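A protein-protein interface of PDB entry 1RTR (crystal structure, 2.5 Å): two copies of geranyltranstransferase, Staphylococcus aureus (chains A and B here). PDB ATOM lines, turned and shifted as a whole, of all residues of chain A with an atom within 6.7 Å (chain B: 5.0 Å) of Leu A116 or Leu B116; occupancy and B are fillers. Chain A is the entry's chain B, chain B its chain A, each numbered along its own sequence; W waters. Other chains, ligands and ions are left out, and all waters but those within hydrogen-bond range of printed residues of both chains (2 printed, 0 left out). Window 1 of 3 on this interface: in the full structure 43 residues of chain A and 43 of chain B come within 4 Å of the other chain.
OG1 of Thr B117 is in hydrogen-bond range of O of Asp B113, 2.6 Å away.
OG1 of Thr A117 sits at hydrogen-bond distance from O of Asp A113, 2.6 Å away.
The backbone carbonyl oxygen (O) of Leu A141 lies within hydrogen-bond range of the side-chain hydroxyl (OG) of Ser A145 (2.8 Å).
The backbone carbonyl oxygen of Ser A145 lies close to the backbone NH of Val A151 (3.3 Å).
Asp A113 touches its own counterpart, Asp B113.
Asp A113 touches Leu B116, and with the chains exchanged Leu A116 touches Asp B113.
Leu A116 touches Thr B117, and with the chains exchanged Thr A117 touches Leu B116.
Phe A120 touches its own counterpart, Phe B120.
Positions printed for both chains: 74, 77, 112, 113, 114, 115, 116, 117, 118, 119 and 120.
Water W2 lies within hydrogen-bond range of the side-chain hydroxyl of Thr B117 (2.8 Å), the backbone carbonyl oxygen of Ser A145 (2.8 Å) and the side-chain hydroxyl of Tyr A77 (2.9 Å).
Water W1 bridges OG1 of Thr A117 and OH of Tyr B77.
Of the 20 printed residues of chain A, 8 touch a printed residue of chain B.
Hydrophobic or aromatic side chains of chain B within 4 Å of the printed part of chain A: Tyr B77, Ala B114, Leu B116 and Phe B120.
Among the printed residues, merely in contact across the chains: Tyr A77 with Asp B113 (3.4 Å), Asp A113 with Tyr B77 (3.1 Å), Asp A113 with Leu B116 (3.8 Å), Leu A116 with Asp B113 (3.7 Å), Leu A116 with Leu B116 (3.4 Å), Leu A116 with Thr B117 (3.7 Å), Thr A117 with Leu B116 (3.6 Å), Phe A120 with Phe B120 (3.8 Å), Ser A145 with Thr B117 (3.9 Å) and Val A151 with Ala B114 (3.7 Å).
The side-chain carboxylate (OD1) of Asp B113 lies within hydrogen-bond range of a ring nitrogen (ND1) of His A81 (2.6 Å).
OD2 of Asp B113 sits close to OD2 of Asp A113, 3.4 Å away.
Leu A116 touches just these residues of chain B: Asp B113, Leu B116 and Thr B117.
Leu B116 touches just these residues of chain A: Asp A113, Leu A116 and Thr A117.
Of the printed residues of chain B, Phe A120 touches Phe B120 (3.8 Å).
Printed residues of chain A within 4 Å of Phe B120: Phe A120.
Of the printed residues of chain A, Asp B113 touches Tyr A77, His A81, Asp A113 and Leu A116.
Of the printed residues of chain A, Tyr B77 touches Asp A113.
Ala A114 touches none of the printed residues of chain B.
Lys A118 touches none of the printed residues of chain B.
The nearest printed residue of chain B that does not touch Leu A116 is Phe B120 (5.7 Å).
The nearest printed residue of chain B that does not touch Ser A145 is Asp B113 (6.0 Å).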
ATOM      1  N   ALA A  70      39.885  -6.829  10.973  1.00  0.00           N
ATOM      2  CA  ALA A  70      38.616  -7.171  10.343  1.00  0.00           C
ATOM      3  C   ALA A  70      38.684  -8.578   9.728  1.00  0.00           C
ATOM      4  O   ALA A  70      37.786  -9.408   9.943  1.00  0.00           O
ATOM      5  CB  ALA A  70      38.254  -6.142   9.292  1.00  0.00           C
ATOM      6  N   MET A  73      38.640 -11.208  12.435  1.00  0.00           N
ATOM      7  CA  MET A  73      37.259 -11.264  12.930  1.00  0.00           C
ATOM      8  C   MET A  73      36.344 -12.083  11.994  1.00  0.00           C
ATOM      9  O   MET A  73      35.500 -12.861  12.457  1.00  0.00           O
ATOM     10  CB  MET A  73      36.690  -9.853  13.065  1.00  0.00           C
ATOM     11  CG  MET A  73      36.935  -9.159  14.395  1.00  0.00           C
ATOM     12  SD  MET A  73      36.314  -7.461  14.352  1.00  0.00           S
ATOM     13  CE  MET A  73      37.178  -6.755  15.711  1.00  0.00           C
ATOM     14  N   ILE A  74      36.496 -11.906  10.679  1.00  0.00           N
ATOM     15  CA  ILE A  74      35.706 -12.700   9.737  1.00  0.00           C
ATOM     16  C   ILE A  74      36.076 -14.174   9.893  1.00  0.00           C
ATOM     17  O   ILE A  74      35.195 -15.057   9.892  1.00  0.00           O
ATOM     18  CB  ILE A  74      35.912 -12.262   8.285  1.00  0.00           C
ATOM     19  CG1 ILE A  74      35.470 -10.814   8.082  1.00  0.00           C
ATOM     20  CG2 ILE A  74      35.204 -13.227   7.338  1.00  0.00           C
ATOM     21  CD1 ILE A  74      34.069 -10.639   7.677  1.00  0.00           C
ATOM     22  N   TYR A  77      34.629 -15.654  13.317  1.00  0.00           N
ATOM     23  CA  TYR A  77      33.179 -15.836  13.304  1.00  0.00           C
ATOM     24  C   TYR A  77      32.758 -17.115  12.574  1.00  0.00           C
ATOM     25  O   TYR A  77      31.840 -17.812  13.027  1.00  0.00           O
ATOM     26  CB  TYR A  77      32.444 -14.608  12.743  1.00  0.00           C
ATOM     27  CG  TYR A  77      31.696 -14.855  11.457  1.00  0.00           C
ATOM     28  CD1 TYR A  77      32.163 -14.337  10.249  1.00  0.00           C
ATOM     29  CD2 TYR A  77      30.534 -15.622  11.434  1.00  0.00           C
ATOM     30  CE1 TYR A  77      31.493 -14.579   9.056  1.00  0.00           C
ATOM     31  CE2 TYR A  77      29.860 -15.864  10.246  1.00  0.00           C
ATOM     32  CZ  TYR A  77      30.342 -15.332   9.071  1.00  0.00           C
ATOM     33  OH  TYR A  77      29.667 -15.554   7.899  1.00  0.00           O
ATOM     34  N   HIS A  81      30.719 -20.335  14.025  1.00  0.00           N
ATOM     35  CA  HIS A  81      29.562 -20.938  13.389  1.00  0.00           C
ATOM     36  C   HIS A  81      29.854 -22.367  12.953  1.00  0.00           C
ATOM     37  O   HIS A  81      28.999 -23.243  13.104  1.00  0.00           O
ATOM     38  CB  HIS A  81      29.037 -20.064  12.247  1.00  0.00           C
ATOM     39  CG  HIS A  81      28.192 -18.913  12.710  1.00  0.00           C
ATOM     40  ND1 HIS A  81      27.428 -18.154  11.851  1.00  0.00           N
ATOM     41  CD2 HIS A  81      27.998 -18.389  13.945  1.00  0.00           C
ATOM     42  CE1 HIS A  81      26.793 -17.219  12.533  1.00  0.00           C
ATOM     43  NE2 HIS A  81      27.125 -17.337  13.805  1.00  0.00           N
ATOM     44  N   ALA A 111      27.595 -14.162  18.885  1.00  0.00           N
ATOM     45  CA  ALA A 111      28.980 -13.685  18.889  1.00  0.00           C
ATOM     46  C   ALA A 111      29.534 -13.654  17.469  1.00  0.00           C
ATOM     47  O   ALA A 111      30.217 -12.705  17.080  1.00  0.00           O
ATOM     48  CB  ALA A 111      29.854 -14.517  19.813  1.00  0.00           C
ATOM     49  N   GLY A 112      29.204 -14.690  16.698  1.00  0.00           N
ATOM     50  CA  GLY A 112      29.544 -14.768  15.285  1.00  0.00           C
ATOM     51  C   GLY A 112      28.940 -13.667  14.427  1.00  0.00           C
ATOM     52  O   GLY A 112      29.661 -12.993  13.681  1.00  0.00           O
ATOM     53  N   ASP A 113      27.626 -13.477  14.527  1.00  0.00           N
ATOM     54  CA  ASP A 113      26.951 -12.395  13.809  1.00  0.00           C
ATOM     55  C   ASP A 113      27.590 -11.043  14.146  1.00  0.00           C
ATOM     56  O   ASP A 113      27.844 -10.208  13.250  1.00  0.00           O
ATOM     57  CB  ASP A 113      25.457 -12.377  14.135  1.00  0.00           C
ATOM     58  CG  ASP A 113      24.731 -13.640  13.665  1.00  0.00           C
ATOM     59  OD1 ASP A 113      23.603 -13.900  14.149  1.00  0.00           O
ATOM     60  OD2 ASP A 113      25.196 -14.439  12.824  1.00  0.00           O
ATOM     61  N   ALA A 114      27.869 -10.840  15.434  1.00  0.00           N
ATOM     62  CA  ALA A 114      28.420  -9.575  15.910  1.00  0.00           C
ATOM     63  C   ALA A 114      29.804  -9.343  15.325  1.00  0.00           C
ATOM     64  O   ALA A 114      30.098  -8.241  14.833  1.00  0.00           O
ATOM     65  CB  ALA A 114      28.457  -9.535  17.448  1.00  0.00           C
ATOM     66  N   LEU A 115      30.635 -10.386  15.345  1.00  0.00           N
ATOM     67  CA  LEU A 115      31.986 -10.312  14.776  1.00  0.00           C
ATOM     68  C   LEU A 115      31.983 -10.032  13.282  1.00  0.00           C
ATOM     69  O   LEU A 115      32.741  -9.178  12.818  1.00  0.00           O
ATOM     70  CB  LEU A 115      32.798 -11.572  15.086  1.00  0.00           C
ATOM     71  CG  LEU A 115      33.380 -11.672  16.503  1.00  0.00           C
ATOM     72  CD1 LEU A 115      33.901 -13.083  16.767  1.00  0.00           C
ATOM     73  CD2 LEU A 115      34.464 -10.658  16.718  1.00  0.00           C
ATOM     74  N   LEU A 116      31.122 -10.734  12.535  1.00  0.00           N
ATOM     75  CA  LEU A 116      30.911 -10.430  11.130  1.00  0.00           C
ATOM     76  C   LEU A 116      30.658  -8.931  10.955  1.00  0.00           C
ATOM     77  O   LEU A 116      31.317  -8.272  10.143  1.00  0.00           O
ATOM     78  CB  LEU A 116      29.719 -11.228  10.560  1.00  0.00           C
ATOM     79  CG  LEU A 116      29.746 -11.652   9.079  1.00  0.00           C
ATOM     80  CD1 LEU A 116      28.382 -12.137   8.538  1.00  0.00           C
ATOM     81  CD2 LEU A 116      30.325 -10.607   8.142  1.00  0.00           C
ATOM     82  N   THR A 117      29.708  -8.410  11.734  1.00  0.00           N
ATOM     83  CA  THR A 117      29.281  -7.021  11.625  1.00  0.00           C
ATOM     84  C   THR A 117      30.383  -6.039  12.002  1.00  0.00           C
ATOM     85  O   THR A 117      30.597  -5.040  11.305  1.00  0.00           O
ATOM     86  CB  THR A 117      28.041  -6.798  12.505  1.00  0.00           C
ATOM     87  OG1 THR A 117      27.122  -7.880  12.295  1.00  0.00           O
ATOM     88  CG2 THR A 117      27.269  -5.574  12.056  1.00  0.00           C
ATOM     89  N   LYS A 118      31.082  -6.333  13.101  1.00  0.00           N
ATOM     90  CA  LYS A 118      32.151  -5.460  13.578  1.00  0.00           C
ATOM     91  C   LYS A 118      33.293  -5.310  12.561  1.00  0.00           C
ATOM     92  O   LYS A 118      33.903  -4.238  12.475  1.00  0.00           O
ATOM     93  CB  LYS A 118      32.682  -5.950  14.931  1.00  0.00           C
ATOM     94  CG  LYS A 118      33.791  -5.101  15.518  1.00  0.00           C
ATOM     95  CD  LYS A 118      33.269  -3.790  16.037  1.00  0.00           C
ATOM     96  CE  LYS A 118      34.274  -3.131  16.966  1.00  0.00           C
ATOM     97  NZ  LYS A 118      34.266  -1.661  16.753  1.00  0.00           N
ATOM     98  N   ALA A 119      33.572  -6.371  11.793  1.00  0.00           N
ATOM     99  CA  ALA A 119      34.619  -6.323  10.763  1.00  0.00           C
ATOM    100  C   ALA A 119      34.337  -5.212   9.778  1.00  0.00           C
ATOM    101  O   ALA A 119      35.232  -4.468   9.410  1.00  0.00           O
ATOM    102  CB  ALA A 119      34.761  -7.659  10.034  1.00  0.00           C
ATOM    103  N   PHE A 120      33.081  -5.098   9.359  1.00  0.00           N
ATOM    104  CA  PHE A 120      32.688  -4.057   8.417  1.00  0.00           C
ATOM    105  C   PHE A 120      32.662  -2.673   9.090  1.00  0.00           C
ATOM    106  O   PHE A 120      32.956  -1.667   8.446  1.00  0.00           O
ATOM    107  CB  PHE A 120      31.365  -4.418   7.741  1.00  0.00           C
ATOM    108  CG  PHE A 120      31.473  -5.596   6.809  1.00  0.00           C
ATOM    109  CD1 PHE A 120      30.947  -6.832   7.158  1.00  0.00           C
ATOM    110  CD2 PHE A 120      32.112  -5.474   5.587  1.00  0.00           C
ATOM    111  CE1 PHE A 120      31.055  -7.920   6.301  1.00  0.00           C
ATOM    112  CE2 PHE A 120      32.222  -6.557   4.735  1.00  0.00           C
ATOM    113  CZ  PHE A 120      31.692  -7.779   5.096  1.00  0.00           C
ATOM    114  N   GLU A 121      32.347  -2.629  10.385  1.00  0.00           N
ATOM    115  CA  GLU A 121      32.484  -1.394  11.155  1.00  0.00           C
ATOM    116  C   GLU A 121      33.929  -0.933  11.195  1.00  0.00           C
ATOM    117  O   GLU A 121      34.232   0.232  10.957  1.00  0.00           O
ATOM    118  CB  GLU A 121      31.972  -1.556  12.583  1.00  0.00           C
ATOM    119  CG  GLU A 121      31.549  -0.238  13.188  1.00  0.00           C
ATOM    120  CD  GLU A 121      32.104  -0.014  14.581  1.00  0.00           C
ATOM    121  OE1 GLU A 121      33.203   0.608  14.669  1.00  0.00           O
ATOM    122  OE2 GLU A 121      31.437  -0.439  15.577  1.00  0.00           O
ATOM    123  N   LEU A 141      35.936  -7.513   0.659  1.00  0.00           N
ATOM    124  CA  LEU A 141      35.695  -8.375   1.814  1.00  0.00           C
ATOM    125  C   LEU A 141      34.330  -9.063   1.762  1.00  0.00           C
ATOM    126  O   LEU A 141      34.215 -10.233   2.126  1.00  0.00           O
ATOM    127  CB  LEU A 141      35.856  -7.620   3.133  1.00  0.00           C
ATOM    128  CG  LEU A 141      35.966  -8.526   4.367  1.00  0.00           C
ATOM    129  CD1 LEU A 141      37.110  -9.576   4.231  1.00  0.00           C
ATOM    130  CD2 LEU A 141      36.136  -7.702   5.618  1.00  0.00           C
ATOM    131  N   SER A 145      33.600 -13.095   1.364  1.00  0.00           N
ATOM    132  CA  SER A 145      33.033 -13.725   2.559  1.00  0.00           C
ATOM    133  C   SER A 145      31.634 -14.266   2.353  1.00  0.00           C
ATOM    134  O   SER A 145      31.178 -15.065   3.154  1.00  0.00           O
ATOM    135  CB  SER A 145      33.005 -12.747   3.737  1.00  0.00           C
ATOM    136  OG  SER A 145      34.307 -12.307   4.060  1.00  0.00           O
ATOM    137  N   MET A 150      33.352 -17.349   1.016  1.00  0.00           N
ATOM    138  CA  MET A 150      33.472 -18.180   2.202  1.00  0.00           C
ATOM    139  C   MET A 150      32.212 -18.986   2.508  1.00  0.00           C
ATOM    140  O   MET A 150      32.295 -20.205   2.634  1.00  0.00           O
ATOM    141  CB  MET A 150      33.923 -17.371   3.420  1.00  0.00           C
ATOM    142  CG  MET A 150      34.389 -18.230   4.588  1.00  0.00           C
ATOM    143  SD  MET A 150      34.826 -17.222   6.023  1.00  0.00           S
ATOM    144  CE  MET A 150      33.230 -16.471   6.355  1.00  0.00           C
ATOM    145  N   VAL A 151      31.053 -18.337   2.624  1.00  0.00           N
ATOM    146  CA  VAL A 151      29.876 -19.097   3.071  1.00  0.00           C
ATOM    147  C   VAL A 151      29.347 -20.065   2.020  1.00  0.00           C
ATOM    148  O   VAL A 151      28.939 -21.158   2.370  1.00  0.00           O
ATOM    149  CB  VAL A 151      28.724 -18.261   3.800  1.00  0.00           C
ATOM    150  CG1 VAL A 151      29.140 -16.845   4.130  1.00  0.00           C
ATOM    151  CG2 VAL A 151      27.397 -18.298   3.046  1.00  0.00           C
ATOM    152  N   ILE B  74      19.175  -7.288   6.193  1.00  0.00           N
ATOM    153  CA  ILE B  74      19.576  -7.350   7.595  1.00  0.00           C
ATOM    154  C   ILE B  74      18.420  -7.792   8.479  1.00  0.00           C
ATOM    155  O   ILE B  74      18.597  -8.595   9.395  1.00  0.00           O
ATOM    156  CB  ILE B  74      20.122  -5.993   8.070  1.00  0.00           C
ATOM    157  CG1 ILE B  74      21.364  -5.625   7.262  1.00  0.00           C
ATOM    158  CG2 ILE B  74      20.382  -5.997   9.582  1.00  0.00           C
ATOM    159  CD1 ILE B  74      22.661  -6.043   7.869  1.00  0.00           C
ATOM    160  N   TYR B  77      17.792 -11.584   7.697  1.00  0.00           N
ATOM    161  CA  TYR B  77      18.799 -12.429   8.341  1.00  0.00           C
ATOM    162  C   TYR B  77      18.551 -12.576   9.848  1.00  0.00           C
ATOM    163  O   TYR B  77      18.723 -13.661  10.395  1.00  0.00           O
ATOM    164  CB  TYR B  77      20.235 -11.931   8.057  1.00  0.00           C
ATOM    165  CG  TYR B  77      21.050 -11.598   9.292  1.00  0.00           C
ATOM    166  CD1 TYR B  77      21.565 -12.606  10.120  1.00  0.00           C
ATOM    167  CD2 TYR B  77      21.299 -10.279   9.638  1.00  0.00           C
ATOM    168  CE1 TYR B  77      22.308 -12.295  11.267  1.00  0.00           C
ATOM    169  CE2 TYR B  77      22.041  -9.951  10.789  1.00  0.00           C
ATOM    170  CZ  TYR B  77      22.547 -10.963  11.585  1.00  0.00           C
ATOM    171  OH  TYR B  77      23.278 -10.640  12.699  1.00  0.00           O
ATOM    172  N   GLY B 112      21.458 -16.962   6.604  1.00  0.00           N
ATOM    173  CA  GLY B 112      21.515 -15.753   7.406  1.00  0.00           C
ATOM    174  C   GLY B 112      22.837 -15.029   7.234  1.00  0.00           C
ATOM    175  O   GLY B 112      22.864 -13.845   6.869  1.00  0.00           O
ATOM    176  N   ASP B 113      23.936 -15.744   7.475  1.00  0.00           N
ATOM    177  CA  ASP B 113      25.283 -15.179   7.340  1.00  0.00           C
ATOM    178  C   ASP B 113      25.530 -14.527   5.981  1.00  0.00           C
ATOM    179  O   ASP B 113      26.127 -13.437   5.902  1.00  0.00           O
ATOM    180  CB  ASP B 113      26.326 -16.251   7.599  1.00  0.00           C
ATOM    181  CG  ASP B 113      26.319 -16.717   9.035  1.00  0.00           C
ATOM    182  OD1 ASP B 113      27.013 -17.711   9.357  1.00  0.00           O
ATOM    183  OD2 ASP B 113      25.624 -16.155   9.910  1.00  0.00           O
ATOM    184  N   ALA B 114      25.045 -15.184   4.924  1.00  0.00           N
ATOM    185  CA  ALA B 114      25.198 -14.685   3.581  1.00  0.00           C
ATOM    186  C   ALA B 114      24.424 -13.378   3.391  1.00  0.00           C
ATOM    187  O   ALA B 114      24.912 -12.429   2.755  1.00  0.00           O
ATOM    188  CB  ALA B 114      24.764 -15.752   2.556  1.00  0.00           C
ATOM    189  N   LEU B 115      23.224 -13.310   3.955  1.00  0.00           N
ATOM    190  CA  LEU B 115      22.388 -12.119   3.770  1.00  0.00           C
ATOM    191  C   LEU B 115      23.001 -10.920   4.488  1.00  0.00           C
ATOM    192  O   LEU B 115      23.050  -9.812   3.923  1.00  0.00           O
ATOM    193  CB  LEU B 115      20.947 -12.364   4.223  1.00  0.00           C
ATOM    194  CG  LEU B 115      20.038 -13.133   3.254  1.00  0.00           C
ATOM    195  CD1 LEU B 115      18.905 -13.773   4.017  1.00  0.00           C
ATOM    196  CD2 LEU B 115      19.489 -12.225   2.166  1.00  0.00           C
ATOM    197  N   LEU B 116      23.494 -11.151   5.707  1.00  0.00           N
ATOM    198  CA  LEU B 116      24.254 -10.146   6.419  1.00  0.00           C
ATOM    199  C   LEU B 116      25.385  -9.642   5.542  1.00  0.00           C
ATOM    200  O   LEU B 116      25.515  -8.438   5.316  1.00  0.00           O
ATOM    201  CB  LEU B 116      24.829 -10.723   7.725  1.00  0.00           C
ATOM    202  CG  LEU B 116      24.941  -9.807   8.946  1.00  0.00           C
ATOM    203  CD1 LEU B 116      25.861 -10.362  10.052  1.00  0.00           C
ATOM    204  CD2 LEU B 116      25.330  -8.385   8.585  1.00  0.00           C
ATOM    205  N   THR B 117      26.200 -10.562   5.033  1.00  0.00           N
ATOM    206  CA  THR B 117      27.284 -10.185   4.146  1.00  0.00           C
ATOM    207  C   THR B 117      26.786  -9.424   2.905  1.00  0.00           C
ATOM    208  O   THR B 117      27.356  -8.378   2.547  1.00  0.00           O
ATOM    209  CB  THR B 117      28.085 -11.431   3.737  1.00  0.00           C
ATOM    210  OG1 THR B 117      28.235 -12.290   4.867  1.00  0.00           O
ATOM    211  CG2 THR B 117      29.526 -11.070   3.394  1.00  0.00           C
ATOM    212  N   LYS B 118      25.734  -9.927   2.248  1.00  0.00           N
ATOM    213  CA  LYS B 118      25.263  -9.298   1.007  1.00  0.00           C
ATOM    214  C   LYS B 118      24.837  -7.831   1.207  1.00  0.00           C
ATOM    215  O   LYS B 118      25.065  -6.983   0.336  1.00  0.00           O
ATOM    216  CB  LYS B 118      24.128 -10.115   0.358  1.00  0.00           C
ATOM    217  CG  LYS B 118      23.660  -9.587  -0.991  1.00  0.00           C
ATOM    218  CD  LYS B 118      24.710  -9.766  -2.082  1.00  0.00           C
ATOM    219  CE  LYS B 118      24.084  -9.659  -3.473  1.00  0.00           C
ATOM    220  NZ  LYS B 118      24.895  -8.808  -4.410  1.00  0.00           N
ATOM    221  N   ALA B 119      24.222  -7.543   2.357  1.00  0.00           N
ATOM    222  CA  ALA B 119      23.771  -6.186   2.668  1.00  0.00           C
ATOM    223  C   ALA B 119      24.903  -5.169   2.552  1.00  0.00           C
ATOM    224  O   ALA B 119      24.709  -4.079   2.007  1.00  0.00           O
ATOM    225  CB  ALA B 119      23.117  -6.137   4.051  1.00  0.00           C
ATOM    226  N   PHE B 120      26.090  -5.545   3.033  1.00  0.00           N
ATOM    227  CA  PHE B 120      27.264  -4.681   2.963  1.00  0.00           C
ATOM    228  C   PHE B 120      27.828  -4.551   1.551  1.00  0.00           C
ATOM    229  O   PHE B 120      28.240  -3.462   1.135  1.00  0.00           O
ATOM    230  CB  PHE B 120      28.309  -5.129   3.978  1.00  0.00           C
ATOM    231  CG  PHE B 120      27.871  -4.908   5.390  1.00  0.00           C
ATOM    232  CD1 PHE B 120      27.848  -3.624   5.928  1.00  0.00           C
ATOM    233  CD2 PHE B 120      27.433  -5.961   6.166  1.00  0.00           C
ATOM    234  CE1 PHE B 120      27.418  -3.400   7.224  1.00  0.00           C
ATOM    235  CE2 PHE B 120      26.996  -5.744   7.462  1.00  0.00           C
ATOM    236  CZ  PHE B 120      26.989  -4.458   7.997  1.00  0.00           C
HETATM  237  O   HOH W   1      24.356  -7.946  12.636  1.00  0.00           O
HETATM  238  O   HOH W   2      30.298 -14.000   5.580  1.00  0.00           O
